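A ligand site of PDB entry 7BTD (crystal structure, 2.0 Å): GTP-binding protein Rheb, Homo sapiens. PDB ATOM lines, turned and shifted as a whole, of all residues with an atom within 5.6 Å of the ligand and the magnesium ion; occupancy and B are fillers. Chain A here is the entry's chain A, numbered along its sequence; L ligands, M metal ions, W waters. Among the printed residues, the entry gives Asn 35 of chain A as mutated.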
ATOM      1  N   GLY A  13       0.145  19.823   2.542  1.00  0.00           N
ATOM      2  CA  GLY A  13       0.853  19.611   1.300  1.00  0.00           C
ATOM      3  C   GLY A  13       1.260  20.888   0.608  1.00  0.00           C
ATOM      4  O   GLY A  13       0.964  21.990   1.070  1.00  0.00           O
ATOM      5  N   TYR A  14       1.958  20.725  -0.511  1.00  0.00           N
ATOM      6  CA  TYR A  14       2.393  21.823  -1.362  1.00  0.00           C
ATOM      7  C   TYR A  14       1.190  22.556  -1.969  1.00  0.00           C
ATOM      8  O   TYR A  14       0.064  22.043  -1.968  1.00  0.00           O
ATOM      9  CB  TYR A  14       3.322  21.272  -2.455  1.00  0.00           C
ATOM     10  CG  TYR A  14       3.979  22.312  -3.353  1.00  0.00           C
ATOM     11  CD1 TYR A  14       4.780  23.323  -2.816  1.00  0.00           C
ATOM     12  CD2 TYR A  14       3.793  22.266  -4.737  1.00  0.00           C
ATOM     13  CE1 TYR A  14       5.381  24.266  -3.642  1.00  0.00           C
ATOM     14  CE2 TYR A  14       4.396  23.199  -5.573  1.00  0.00           C
ATOM     15  CZ  TYR A  14       5.186  24.201  -5.019  1.00  0.00           C
ATOM     16  OH  TYR A  14       5.767  25.131  -5.825  1.00  0.00           O
ATOM     17  N   ARG A  15       1.422  23.772  -2.467  1.00  0.00           N
ATOM     18  CA  ARG A  15       0.394  24.573  -3.129  1.00  0.00           C
ATOM     19  C   ARG A  15      -0.163  23.866  -4.367  1.00  0.00           C
ATOM     20  O   ARG A  15       0.583  23.219  -5.093  1.00  0.00           O
ATOM     21  CB  ARG A  15       0.966  25.935  -3.530  1.00  0.00           C
ATOM     22  CG  ARG A  15       1.052  26.913  -2.381  1.00  0.00           C
ATOM     23  CD  ARG A  15       1.649  28.256  -2.809  1.00  0.00           C
ATOM     24  NE  ARG A  15       3.105  28.212  -2.917  1.00  0.00           N
ATOM     25  CZ  ARG A  15       3.957  28.453  -1.920  1.00  0.00           C
ATOM     26  NH1 ARG A  15       3.527  28.774  -0.703  1.00  0.00           N
ATOM     27  NH2 ARG A  15       5.261  28.363  -2.159  1.00  0.00           N
ATOM     28  N   SER A  16      -1.479  23.975  -4.571  1.00  0.00           N
ATOM     29  CA  SER A  16      -2.176  23.509  -5.795  1.00  0.00           C
ATOM     30  C   SER A  16      -2.196  21.993  -6.061  1.00  0.00           C
ATOM     31  O   SER A  16      -2.473  21.582  -7.200  1.00  0.00           O
ATOM     32  CB  SER A  16      -1.637  24.225  -7.052  1.00  0.00           C
ATOM     33  OG  SER A  16      -1.864  25.613  -6.985  1.00  0.00           O
ATOM     34  N   VAL A  17      -1.932  21.186  -5.035  1.00  0.00           N
ATOM     35  CA  VAL A  17      -1.974  19.723  -5.195  1.00  0.00           C
ATOM     36  C   VAL A  17      -3.399  19.158  -5.162  1.00  0.00           C
ATOM     37  O   VAL A  17      -3.633  17.995  -5.518  1.00  0.00           O
ATOM     38  CB  VAL A  17      -1.090  18.970  -4.155  1.00  0.00           C
ATOM     39  CG1 VAL A  17       0.362  19.425  -4.284  1.00  0.00           C
ATOM     40  CG2 VAL A  17      -1.602  19.159  -2.730  1.00  0.00           C
ATOM     41  N   GLY A  18      -4.345  19.995  -4.714  1.00  0.00           N
ATOM     42  CA  GLY A  18      -5.751  19.657  -4.679  1.00  0.00           C
ATOM     43  C   GLY A  18      -6.305  19.321  -3.308  1.00  0.00           C
ATOM     44  O   GLY A  18      -7.278  18.581  -3.199  1.00  0.00           O
ATOM     45  N   LYS A  19      -5.688  19.860  -2.254  1.00  0.00           N
ATOM     46  CA  LYS A  19      -6.132  19.618  -0.876  1.00  0.00           C
ATOM     47  C   LYS A  19      -7.585  20.055  -0.707  1.00  0.00           C
ATOM     48  O   LYS A  19      -8.411  19.289  -0.202  1.00  0.00           O
ATOM     49  CB  LYS A  19      -5.249  20.343   0.153  1.00  0.00           C
ATOM     50  CG  LYS A  19      -3.800  19.861   0.178  1.00  0.00           C
ATOM     51  CD  LYS A  19      -2.942  20.592   1.215  1.00  0.00           C
ATOM     52  CE  LYS A  19      -2.750  22.095   0.946  1.00  0.00           C
ATOM     53  NZ  LYS A  19      -2.258  22.451  -0.418  1.00  0.00           N
ATOM     54  N   SER A  20      -7.903  21.260  -1.176  1.00  0.00           N
ATOM     55  CA  SER A  20      -9.250  21.815  -1.079  1.00  0.00           C
ATOM     56  C   SER A  20     -10.242  21.063  -1.945  1.00  0.00           C
ATOM     57  O   SER A  20     -11.335  20.733  -1.473  1.00  0.00           O
ATOM     58  CB  SER A  20      -9.281  23.299  -1.459  1.00  0.00           C
ATOM     59  OG  SER A  20      -8.560  24.063  -0.497  1.00  0.00           O
ATOM     60  N   SER A  21      -9.857  20.773  -3.185  1.00  0.00           N
ATOM     61  CA  SER A  21     -10.728  20.065  -4.114  1.00  0.00           C
ATOM     62  C   SER A  21     -11.066  18.650  -3.625  1.00  0.00           C
ATOM     63  O   SER A  21     -12.194  18.211  -3.767  1.00  0.00           O
ATOM     64  CB  SER A  21     -10.125  20.029  -5.516  1.00  0.00           C
ATOM     65  OG  SER A  21      -9.876  21.339  -5.984  1.00  0.00           O
ATOM     66  N   LEU A  22     -10.074  17.959  -3.047  1.00  0.00           N
ATOM     67  CA  LEU A  22     -10.303  16.634  -2.453  1.00  0.00           C
ATOM     68  C   LEU A  22     -11.252  16.680  -1.263  1.00  0.00           C
ATOM     69  O   LEU A  22     -12.169  15.870  -1.160  1.00  0.00           O
ATOM     70  CB  LEU A  22      -8.996  15.986  -2.019  1.00  0.00           C
ATOM     71  CG  LEU A  22      -8.357  14.830  -2.779  1.00  0.00           C
ATOM     72  CD1 LEU A  22      -7.136  14.352  -2.002  1.00  0.00           C
ATOM     73  CD2 LEU A  22      -9.311  13.664  -3.047  1.00  0.00           C
ATOM     74  N   PHE A  31     -17.057  18.530  -7.586  1.00  0.00           N
ATOM     75  CA  PHE A  31     -15.726  19.023  -7.960  1.00  0.00           C
ATOM     76  C   PHE A  31     -15.738  20.495  -8.345  1.00  0.00           C
ATOM     77  O   PHE A  31     -16.487  20.901  -9.236  1.00  0.00           O
ATOM     78  CB  PHE A  31     -15.108  18.153  -9.062  1.00  0.00           C
ATOM     79  CG  PHE A  31     -13.800  18.696  -9.600  1.00  0.00           C
ATOM     80  CD1 PHE A  31     -12.643  18.689  -8.817  1.00  0.00           C
ATOM     81  CD2 PHE A  31     -13.733  19.215 -10.895  1.00  0.00           C
ATOM     82  CE1 PHE A  31     -11.442  19.185  -9.318  1.00  0.00           C
ATOM     83  CE2 PHE A  31     -12.535  19.710 -11.405  1.00  0.00           C
ATOM     84  CZ  PHE A  31     -11.386  19.698 -10.619  1.00  0.00           C
ATOM     85  N   VAL A  32     -14.875  21.279  -7.698  1.00  0.00           N
ATOM     86  CA  VAL A  32     -14.705  22.710  -7.978  1.00  0.00           C
ATOM     87  C   VAL A  32     -13.510  22.968  -8.917  1.00  0.00           C
ATOM     88  O   VAL A  32     -12.360  22.698  -8.555  1.00  0.00           O
ATOM     89  CB  VAL A  32     -14.592  23.533  -6.667  1.00  0.00           C
ATOM     90  CG1 VAL A  32     -14.469  25.017  -6.973  1.00  0.00           C
ATOM     91  CG2 VAL A  32     -15.805  23.301  -5.782  1.00  0.00           C
ATOM     92  N   ASP A  33     -13.812  23.506 -10.093  1.00  0.00           N
ATOM     93  CA  ASP A  33     -12.859  23.698 -11.190  1.00  0.00           C
ATOM     94  C   ASP A  33     -11.699  24.663 -10.882  1.00  0.00           C
ATOM     95  O   ASP A  33     -10.605  24.521 -11.434  1.00  0.00           O
ATOM     96  CB  ASP A  33     -13.603  24.180 -12.444  1.00  0.00           C
ATOM     97  CG  ASP A  33     -12.988  23.647 -13.730  1.00  0.00           C
ATOM     98  OD1 ASP A  33     -13.721  22.974 -14.489  1.00  0.00           O
ATOM     99  OD2 ASP A  33     -11.791  23.894 -13.996  1.00  0.00           O
ATOM    100  N   SER A  34     -11.953  25.647 -10.022  1.00  0.00           N
ATOM    101  CA  SER A  34     -10.903  26.571  -9.568  1.00  0.00           C
ATOM    102  C   SER A  34     -11.242  27.111  -8.189  1.00  0.00           C
ATOM    103  O   SER A  34     -12.378  27.524  -7.935  1.00  0.00           O
ATOM    104  CB  SER A  34     -10.682  27.716 -10.578  1.00  0.00           C
ATOM    105  OG  SER A  34     -11.717  28.723 -10.478  1.00  0.00           O
ATOM    106  N   ASN A  35     -10.252  27.077  -7.308  1.00  0.00           N
ATOM    107  CA  ASN A  35     -10.408  27.521  -5.922  1.00  0.00           C
ATOM    108  C   ASN A  35      -9.482  28.682  -5.665  1.00  0.00           C
ATOM    109  O   ASN A  35      -8.480  28.855  -6.376  1.00  0.00           O
ATOM    110  CB  ASN A  35     -10.063  26.386  -4.935  1.00  0.00           C
ATOM    111  CG  ASN A  35     -10.839  25.107  -5.179  1.00  0.00           C
ATOM    112  OD1 ASN A  35     -11.805  24.814  -4.480  1.00  0.00           O
ATOM    113  ND2 ASN A  35     -10.415  24.333  -6.176  1.00  0.00           N
ATOM    114  N   ASP A  36      -9.814  29.504  -4.679  1.00  0.00           N
ATOM    115  CA  ASP A  36      -8.848  30.429  -4.109  1.00  0.00           C
ATOM    116  C   ASP A  36      -7.763  29.615  -3.400  1.00  0.00           C
ATOM    117  O   ASP A  36      -8.065  28.543  -2.851  1.00  0.00           O
ATOM    118  CB  ASP A  36      -9.506  31.372  -3.094  1.00  0.00           C
ATOM    119  CG  ASP A  36     -10.417  32.403  -3.736  1.00  0.00           C
ATOM    120  OD1 ASP A  36     -10.433  32.521  -4.976  1.00  0.00           O
ATOM    121  OD2 ASP A  36     -11.111  33.107  -2.986  1.00  0.00           O
ATOM    122  N   PRO A  37      -6.499  30.099  -3.423  1.00  0.00           N
ATOM    123  CA  PRO A  37      -5.506  29.541  -2.504  1.00  0.00           C
ATOM    124  C   PRO A  37      -6.000  29.634  -1.067  1.00  0.00           C
ATOM    125  O   PRO A  37      -6.558  30.665  -0.679  1.00  0.00           O
ATOM    126  CB  PRO A  37      -4.274  30.440  -2.718  1.00  0.00           C
ATOM    127  CG  PRO A  37      -4.706  31.563  -3.606  1.00  0.00           C
ATOM    128  CD  PRO A  37      -5.911  31.085  -4.351  1.00  0.00           C
ATOM    129  N   THR A  38      -5.822  28.566  -0.304  1.00  0.00           N
ATOM    130  CA  THR A  38      -6.425  28.462   1.017  1.00  0.00           C
ATOM    131  C   THR A  38      -5.620  29.243   2.042  1.00  0.00           C
ATOM    132  O   THR A  38      -4.396  29.335   1.938  1.00  0.00           O
ATOM    133  CB  THR A  38      -6.558  26.979   1.435  1.00  0.00           C
ATOM    134  OG1 THR A  38      -7.317  26.298   0.427  1.00  0.00           O
ATOM    135  CG2 THR A  38      -7.237  26.788   2.800  1.00  0.00           C
ATOM    136  N   ASP A  60      -8.502  22.015   6.410  1.00  0.00           N
ATOM    137  CA  ASP A  60      -7.912  22.206   5.099  1.00  0.00           C
ATOM    138  C   ASP A  60      -6.934  23.382   5.193  1.00  0.00           C
ATOM    139  O   ASP A  60      -7.345  24.525   5.451  1.00  0.00           O
ATOM    140  CB  ASP A  60      -9.013  22.449   4.065  1.00  0.00           C
ATOM    141  CG  ASP A  60      -8.482  22.676   2.659  1.00  0.00           C
ATOM    142  OD1 ASP A  60      -7.423  22.123   2.298  1.00  0.00           O
ATOM    143  OD2 ASP A  60      -9.151  23.426   1.920  1.00  0.00           O
ATOM    144  N   THR A  61      -5.654  23.085   4.993  1.00  0.00           N
ATOM    145  CA  THR A  61      -4.580  24.043   5.302  1.00  0.00           C
ATOM    146  C   THR A  61      -4.023  24.769   4.069  1.00  0.00           C
ATOM    147  O   THR A  61      -4.275  24.362   2.932  1.00  0.00           O
ATOM    148  CB  THR A  61      -3.424  23.368   6.077  1.00  0.00           C
ATOM    149  OG1 THR A  61      -2.736  22.438   5.222  1.00  0.00           O
ATOM    150  CG2 THR A  61      -3.952  22.613   7.305  1.00  0.00           C
ATOM    151  N   ALA A  62      -3.290  25.853   4.303  1.00  0.00           N
ATOM    152  CA  ALA A  62      -2.583  26.563   3.247  1.00  0.00           C
ATOM    153  C   ALA A  62      -1.432  25.707   2.717  1.00  0.00           C
ATOM    154  O   ALA A  62      -0.729  25.049   3.491  1.00  0.00           O
ATOM    155  CB  ALA A  62      -2.054  27.899   3.775  1.00  0.00           C
ATOM    156  N   GLY A  63      -1.243  25.710   1.394  1.00  0.00           N
ATOM    157  CA  GLY A  63      -0.079  25.067   0.785  1.00  0.00           C
ATOM    158  C   GLY A  63       1.225  25.542   1.409  1.00  0.00           C
ATOM    159  O   GLY A  63       1.390  26.722   1.700  1.00  0.00           O
ATOM    160  N   GLN A  64       2.124  24.601   1.648  1.00  0.00           N
ATOM    161  CA  GLN A  64       3.454  24.904   2.199  1.00  0.00           C
ATOM    162  C   GLN A  64       4.520  24.547   1.169  1.00  0.00           C
ATOM    163  O   GLN A  64       4.310  23.667   0.348  1.00  0.00           O
ATOM    164  CB  GLN A  64       3.700  24.123   3.487  1.00  0.00           C
ATOM    165  CG  GLN A  64       2.760  24.475   4.634  1.00  0.00           C
ATOM    166  CD  GLN A  64       2.987  23.600   5.861  1.00  0.00           C
ATOM    167  OE1 GLN A  64       4.113  23.430   6.309  1.00  0.00           O
ATOM    168  NE2 GLN A  64       1.917  23.067   6.419  1.00  0.00           N
ATOM    169  N   ASN A 119      -2.664  12.785  -5.541  1.00  0.00           N
ATOM    170  CA  ASN A 119      -3.866  13.306  -6.172  1.00  0.00           C
ATOM    171  C   ASN A 119      -3.670  13.618  -7.668  1.00  0.00           C
ATOM    172  O   ASN A 119      -2.533  13.537  -8.182  1.00  0.00           O
ATOM    173  CB  ASN A 119      -4.333  14.548  -5.393  1.00  0.00           C
ATOM    174  CG  ASN A 119      -5.750  14.968  -5.753  1.00  0.00           C
ATOM    175  OD1 ASN A 119      -6.671  14.150  -5.852  1.00  0.00           O
ATOM    176  ND2 ASN A 119      -5.933  16.274  -5.945  1.00  0.00           N
ATOM    177  N   LYS A 120      -4.772  13.955  -8.341  1.00  0.00           N
ATOM    178  CA  LYS A 120      -4.823  14.295  -9.775  1.00  0.00           C
ATOM    179  C   LYS A 120      -4.521  13.094 -10.674  1.00  0.00           C
ATOM    180  O   LYS A 120      -3.993  13.260 -11.775  1.00  0.00           O
ATOM    181  CB  LYS A 120      -3.900  15.489 -10.140  1.00  0.00           C
ATOM    182  CG  LYS A 120      -4.125  16.743  -9.300  1.00  0.00           C
ATOM    183  CD  LYS A 120      -3.548  17.986  -9.983  1.00  0.00           C
ATOM    184  CE  LYS A 120      -3.699  19.201  -9.075  1.00  0.00           C
ATOM    185  NZ  LYS A 120      -3.142  20.452  -9.655  1.00  0.00           N
ATOM    186  N   LYS A 121      -4.888  11.887 -10.227  1.00  0.00           N
ATOM    187  CA  LYS A 121      -4.601  10.659 -10.985  1.00  0.00           C
ATOM    188  C   LYS A 121      -5.387  10.591 -12.299  1.00  0.00           C
ATOM    189  O   LYS A 121      -5.069   9.793 -13.176  1.00  0.00           O
ATOM    190  CB  LYS A 121      -4.823   9.389 -10.145  1.00  0.00           C
ATOM    191  CG  LYS A 121      -6.281   8.965  -9.988  1.00  0.00           C
ATOM    192  CD  LYS A 121      -6.419   7.770  -9.063  1.00  0.00           C
ATOM    193  CE  LYS A 121      -7.859   7.289  -8.997  1.00  0.00           C
ATOM    194  NZ  LYS A 121      -8.309   6.615 -10.237  1.00  0.00           N
ATOM    195  N   ASP A 122      -6.414  11.434 -12.429  1.00  0.00           N
ATOM    196  CA  ASP A 122      -7.185  11.516 -13.670  1.00  0.00           C
ATOM    197  C   ASP A 122      -6.401  12.184 -14.811  1.00  0.00           C
ATOM    198  O   ASP A 122      -6.728  12.015 -15.990  1.00  0.00           O
ATOM    199  CB  ASP A 122      -8.508  12.273 -13.438  1.00  0.00           C
ATOM    200  CG  ASP A 122      -8.296  13.689 -12.918  1.00  0.00           C
ATOM    201  OD1 ASP A 122      -7.897  13.845 -11.742  1.00  0.00           O
ATOM    202  OD2 ASP A 122      -8.533  14.637 -13.702  1.00  0.00           O
ATOM    203  N   LEU A 123      -5.345  12.925 -14.464  1.00  0.00           N
ATOM    204  CA  LEU A 123      -4.553  13.652 -15.457  1.00  0.00           C
ATOM    205  C   LEU A 123      -3.425  12.769 -16.016  1.00  0.00           C
ATOM    206  O   LEU A 123      -2.244  13.010 -15.745  1.00  0.00           O
ATOM    207  CB  LEU A 123      -4.029  14.982 -14.894  1.00  0.00           C
ATOM    208  CG  LEU A 123      -5.079  16.028 -14.482  1.00  0.00           C
ATOM    209  CD1 LEU A 123      -4.393  17.246 -13.847  1.00  0.00           C
ATOM    210  CD2 LEU A 123      -5.993  16.445 -15.640  1.00  0.00           C
ATOM    211  N   SER A 148      -5.676   9.414  -5.687  1.00  0.00           N
ATOM    212  CA  SER A 148      -7.010   9.982  -5.705  1.00  0.00           C
ATOM    213  C   SER A 148      -7.189  10.910  -6.895  1.00  0.00           C
ATOM    214  O   SER A 148      -6.216  11.324  -7.524  1.00  0.00           O
ATOM    215  CB  SER A 148      -7.262  10.761  -4.405  1.00  0.00           C
ATOM    216  OG  SER A 148      -6.411  11.916  -4.336  1.00  0.00           O
ATOM    217  N   SER A 149      -8.449  11.202  -7.189  1.00  0.00           N
ATOM    218  CA  SER A 149      -8.803  12.315  -8.038  1.00  0.00           C
ATOM    219  C   SER A 149      -9.945  13.053  -7.359  1.00  0.00           C
ATOM    220  O   SER A 149     -10.943  12.429  -6.961  1.00  0.00           O
ATOM    221  CB  SER A 149      -9.241  11.832  -9.417  1.00  0.00           C
ATOM    222  OG  SER A 149      -9.854  12.891 -10.129  1.00  0.00           O
ATOM    223  N   ALA A 150      -9.805  14.378  -7.239  1.00  0.00           N
ATOM    224  CA  ALA A 150     -10.861  15.224  -6.689  1.00  0.00           C
ATOM    225  C   ALA A 150     -12.111  15.246  -7.560  1.00  0.00           C
ATOM    226  O   ALA A 150     -13.151  15.738  -7.140  1.00  0.00           O
ATOM    227  CB  ALA A 150     -10.351  16.642  -6.483  1.00  0.00           C
ATOM    228  N   LYS A 151     -12.001  14.718  -8.783  1.00  0.00           N
ATOM    229  CA  LYS A 151     -13.144  14.548  -9.698  1.00  0.00           C
ATOM    230  C   LYS A 151     -13.931  13.256  -9.428  1.00  0.00           C
ATOM    231  O   LYS A 151     -15.023  13.070  -9.969  1.00  0.00           O
ATOM    232  CB  LYS A 151     -12.653  14.538 -11.162  1.00  0.00           C
ATOM    233  CG  LYS A 151     -12.275  15.899 -11.719  1.00  0.00           C
ATOM    234  CD  LYS A 151     -11.942  15.775 -13.211  1.00  0.00           C
ATOM    235  CE  LYS A 151     -11.793  17.146 -13.850  1.00  0.00           C
ATOM    236  NZ  LYS A 151     -11.709  17.051 -15.333  1.00  0.00           N
HETATM  237  P1  LIG L   1      -3.624  25.706  -1.854  1.00  0.00           P
HETATM  238  O1  LIG L   1      -3.152  27.008  -2.380  1.00  0.00           O
HETATM  239  O2  LIG L   1      -4.809  25.905  -0.858  1.00  0.00           O
HETATM  240  O3  LIG L   1      -2.422  24.969  -1.148  1.00  0.00           O
HETATM  241  N1  LIG L   1      -4.100  24.780  -3.197  1.00  0.00           N
HETATM  242  P2  LIG L   1      -4.865  23.267  -3.021  1.00  0.00           P
HETATM  243  O4  LIG L   1      -3.913  22.200  -2.635  1.00  0.00           O
HETATM  244  O5  LIG L   1      -6.074  23.391  -2.044  1.00  0.00           O
HETATM  245  O6  LIG L   1      -5.361  22.904  -4.489  1.00  0.00           O
HETATM  246  P3  LIG L   1      -6.821  23.208  -5.037  1.00  0.00           P
HETATM  247  O7  LIG L   1      -7.803  22.218  -4.442  1.00  0.00           O
HETATM  248  O8  LIG L   1      -7.132  24.659  -4.952  1.00  0.00           O
HETATM  249  O9  LIG L   1      -6.628  22.793  -6.572  1.00  0.00           O
HETATM  250  C1  LIG L   1      -5.683  23.447  -7.433  1.00  0.00           C
HETATM  251  C2  LIG L   1      -6.155  23.326  -8.894  1.00  0.00           C
HETATM  252  O10 LIG L   1      -6.077  21.949  -9.299  1.00  0.00           O
HETATM  253  C3  LIG L   1      -7.610  23.728  -9.117  1.00  0.00           C
HETATM  254  O11 LIG L   1      -7.701  24.311 -10.411  1.00  0.00           O
HETATM  255  C4  LIG L   1      -8.363  22.405  -9.058  1.00  0.00           C
HETATM  256  O12 LIG L   1      -9.610  22.398  -9.752  1.00  0.00           O
HETATM  257  C5  LIG L   1      -7.357  21.446  -9.677  1.00  0.00           C
HETATM  258  N2  LIG L   1      -7.455  20.076  -9.143  1.00  0.00           N
HETATM  259  C6  LIG L   1      -7.391  19.700  -7.836  1.00  0.00           C
HETATM  260  N3  LIG L   1      -7.507  18.370  -7.704  1.00  0.00           N
HETATM  261  C7  LIG L   1      -7.648  17.871  -8.950  1.00  0.00           C
HETATM  262  C8  LIG L   1      -7.798  16.520  -9.494  1.00  0.00           C
HETATM  263  O13 LIG L   1      -7.830  15.530  -8.735  1.00  0.00           O
HETATM  264  N4  LIG L   1      -7.895  16.423 -10.846  1.00  0.00           N
HETATM  265  C9  LIG L   1      -7.869  17.506 -11.676  1.00  0.00           C
HETATM  266  N5  LIG L   1      -7.995  17.318 -12.999  1.00  0.00           N
HETATM  267  N6  LIG L   1      -7.713  18.771 -11.236  1.00  0.00           N
HETATM  268  C10 LIG L   1      -7.598  18.974  -9.890  1.00  0.00           C
HETATM  269 MG    MG M   1      -6.550  24.876  -0.878  1.00  0.00          MG
HETATM  270  O   HOH W   1      -5.144  26.741  -5.565  1.00  0.00           O
HETATM  271  O   HOH W   2      -8.662  19.392 -15.083  1.00  0.00           O
HETATM  272  O   HOH W   3      -7.462  25.920  -2.583  1.00  0.00           O
HETATM  273  O   HOH W   4      -2.699  27.567  -4.786  1.00  0.00           O
HETATM  274  O   HOH W   5      -5.872  23.776   0.803  1.00  0.00           O
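A nitrogen (N4) of the ligand sits at hydrogen-bond distance from the side-chain carboxylate (OD1) of Asp 122 (2.7 Å). An oxygen (O13) of the ligand lies within hydrogen-bond range of the backbone NH of Ala 150, 2.7 Å away. N of Gly 18 sits at hydrogen-bond distance from O4 of the ligand, 3.1 Å away. O2 of the ligand sits close to N of Thr 38, 2.9 Å away. O12 of the ligand sits at hydrogen-bond distance from O of Val 32. The backbone NH of Ser 21 sits at hydrogen-bond distance from an oxygen (O7) of the ligand. OG of Ser 21 lies within hydrogen-bond range of O7 of the ligand, 2.7 Å away. The side-chain amino group (NZ) of Lys 19 is in salt-bridge range of an oxygen (O3) of the ligand, at 2.6 Å. N of Ser 20 is in hydrogen-bond range of O7 of the ligand, at 3.4 Å. The backbone NH (N) of Gly 63 lies within hydrogen-bond range of an oxygen (O3) of the ligand (2.9 Å). The backbone NH of Lys 120 sits close to an oxygen (O13) of the ligand (3.5 Å). The side-chain amide nitrogen of Asn 119 sits at hydrogen-bond distance from a nitrogen (N3) of the ligand, 3.2 Å away. An oxygen (O4) of the ligand lies within hydrogen-bond range of the backbone NH of Lys 19 (3.0 Å). An oxygen (O12) of the ligand sits at hydrogen-bond distance from the backbone carbonyl oxygen (O) of Asp 33 (2.9 Å). An oxygen (O4) of the ligand is in hydrogen-bond range of the backbone NH of Val 17 (3.3 Å). NZ of Lys 120 is in hydrogen-bond range of O10 of the ligand, at 3.3 Å.
The side-chain amino group of Lys 120 is in hydrogen-bond range of the backbone carbonyl oxygen of Ser 16, 2.8 Å away. OG of Ser 20 sits close to OD2 of Asp 60 (2.6 Å). The side-chain hydroxyl of Ser 21 is in hydrogen-bond range of the side-chain amide nitrogen of Asn 35, at 3.0 Å. N of Ala 150 sits at hydrogen-bond distance from OD1 of Asn 119 (3.4 Å). The side-chain hydroxyl (OG) of Ser 148 is in hydrogen-bond range of the side-chain amide oxygen (OD1) of Asn 119. The backbone NH (N) of Lys 151 lies close to the side-chain hydroxyl (OG) of Ser 149, at 3.1 Å. ND2 of Asn 119 sits at hydrogen-bond distance from O of Val 17, at 2.9 Å. OD1 of Asp 122 sits at hydrogen-bond distance from OG of Ser 149, 2.7 Å away.
A nitrogen (N1) of the ligand lies close to the backbone NH of Ser 16 (3.1 Å). Tyr 14 touches the ligand. CA of Arg 15 touches O3 of the ligand (3.5 Å). Phe 31 touches the ligand (CZ to O12, 3.3 Å). CB of Asn 35 touches O8 of the ligand, 3.4 Å away. Pro 37 touches the ligand. Leu 123 touches the ligand (CD2 to N5, 3.4 Å). Ser 149 touches the ligand. CE of Lys 151 touches N5 of the ligand, at 3.9 Å. Of the 32 residues printed, 22 come within 4 Å of the ligand. The nearest printed residue that does not touch the ligand is Ser 34 (4.01 Å).
Of the 32 residues printed, 2 come within 4 Å of the magnesium ion.
The magnesium ion is bound by O5 of the ligand, O2 of the ligand, OG1 of Thr 38, water W5, water W3 and OG of Ser 20. The magnesium ion has six donor atoms within binding distance.
Water W5 bridges OD1 of Asp 60 (2.7 Å) and O of Thr 61 (2.7 Å). Water W3 bridges the backbone carbonyl oxygen (O) of Asp 36 (2.7 Å) and an oxygen (O8) of the ligand (2.7 Å). Water W4 bridges O1 of the ligand (2.5 Å) and OG of Ser 16 (3.1 Å).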
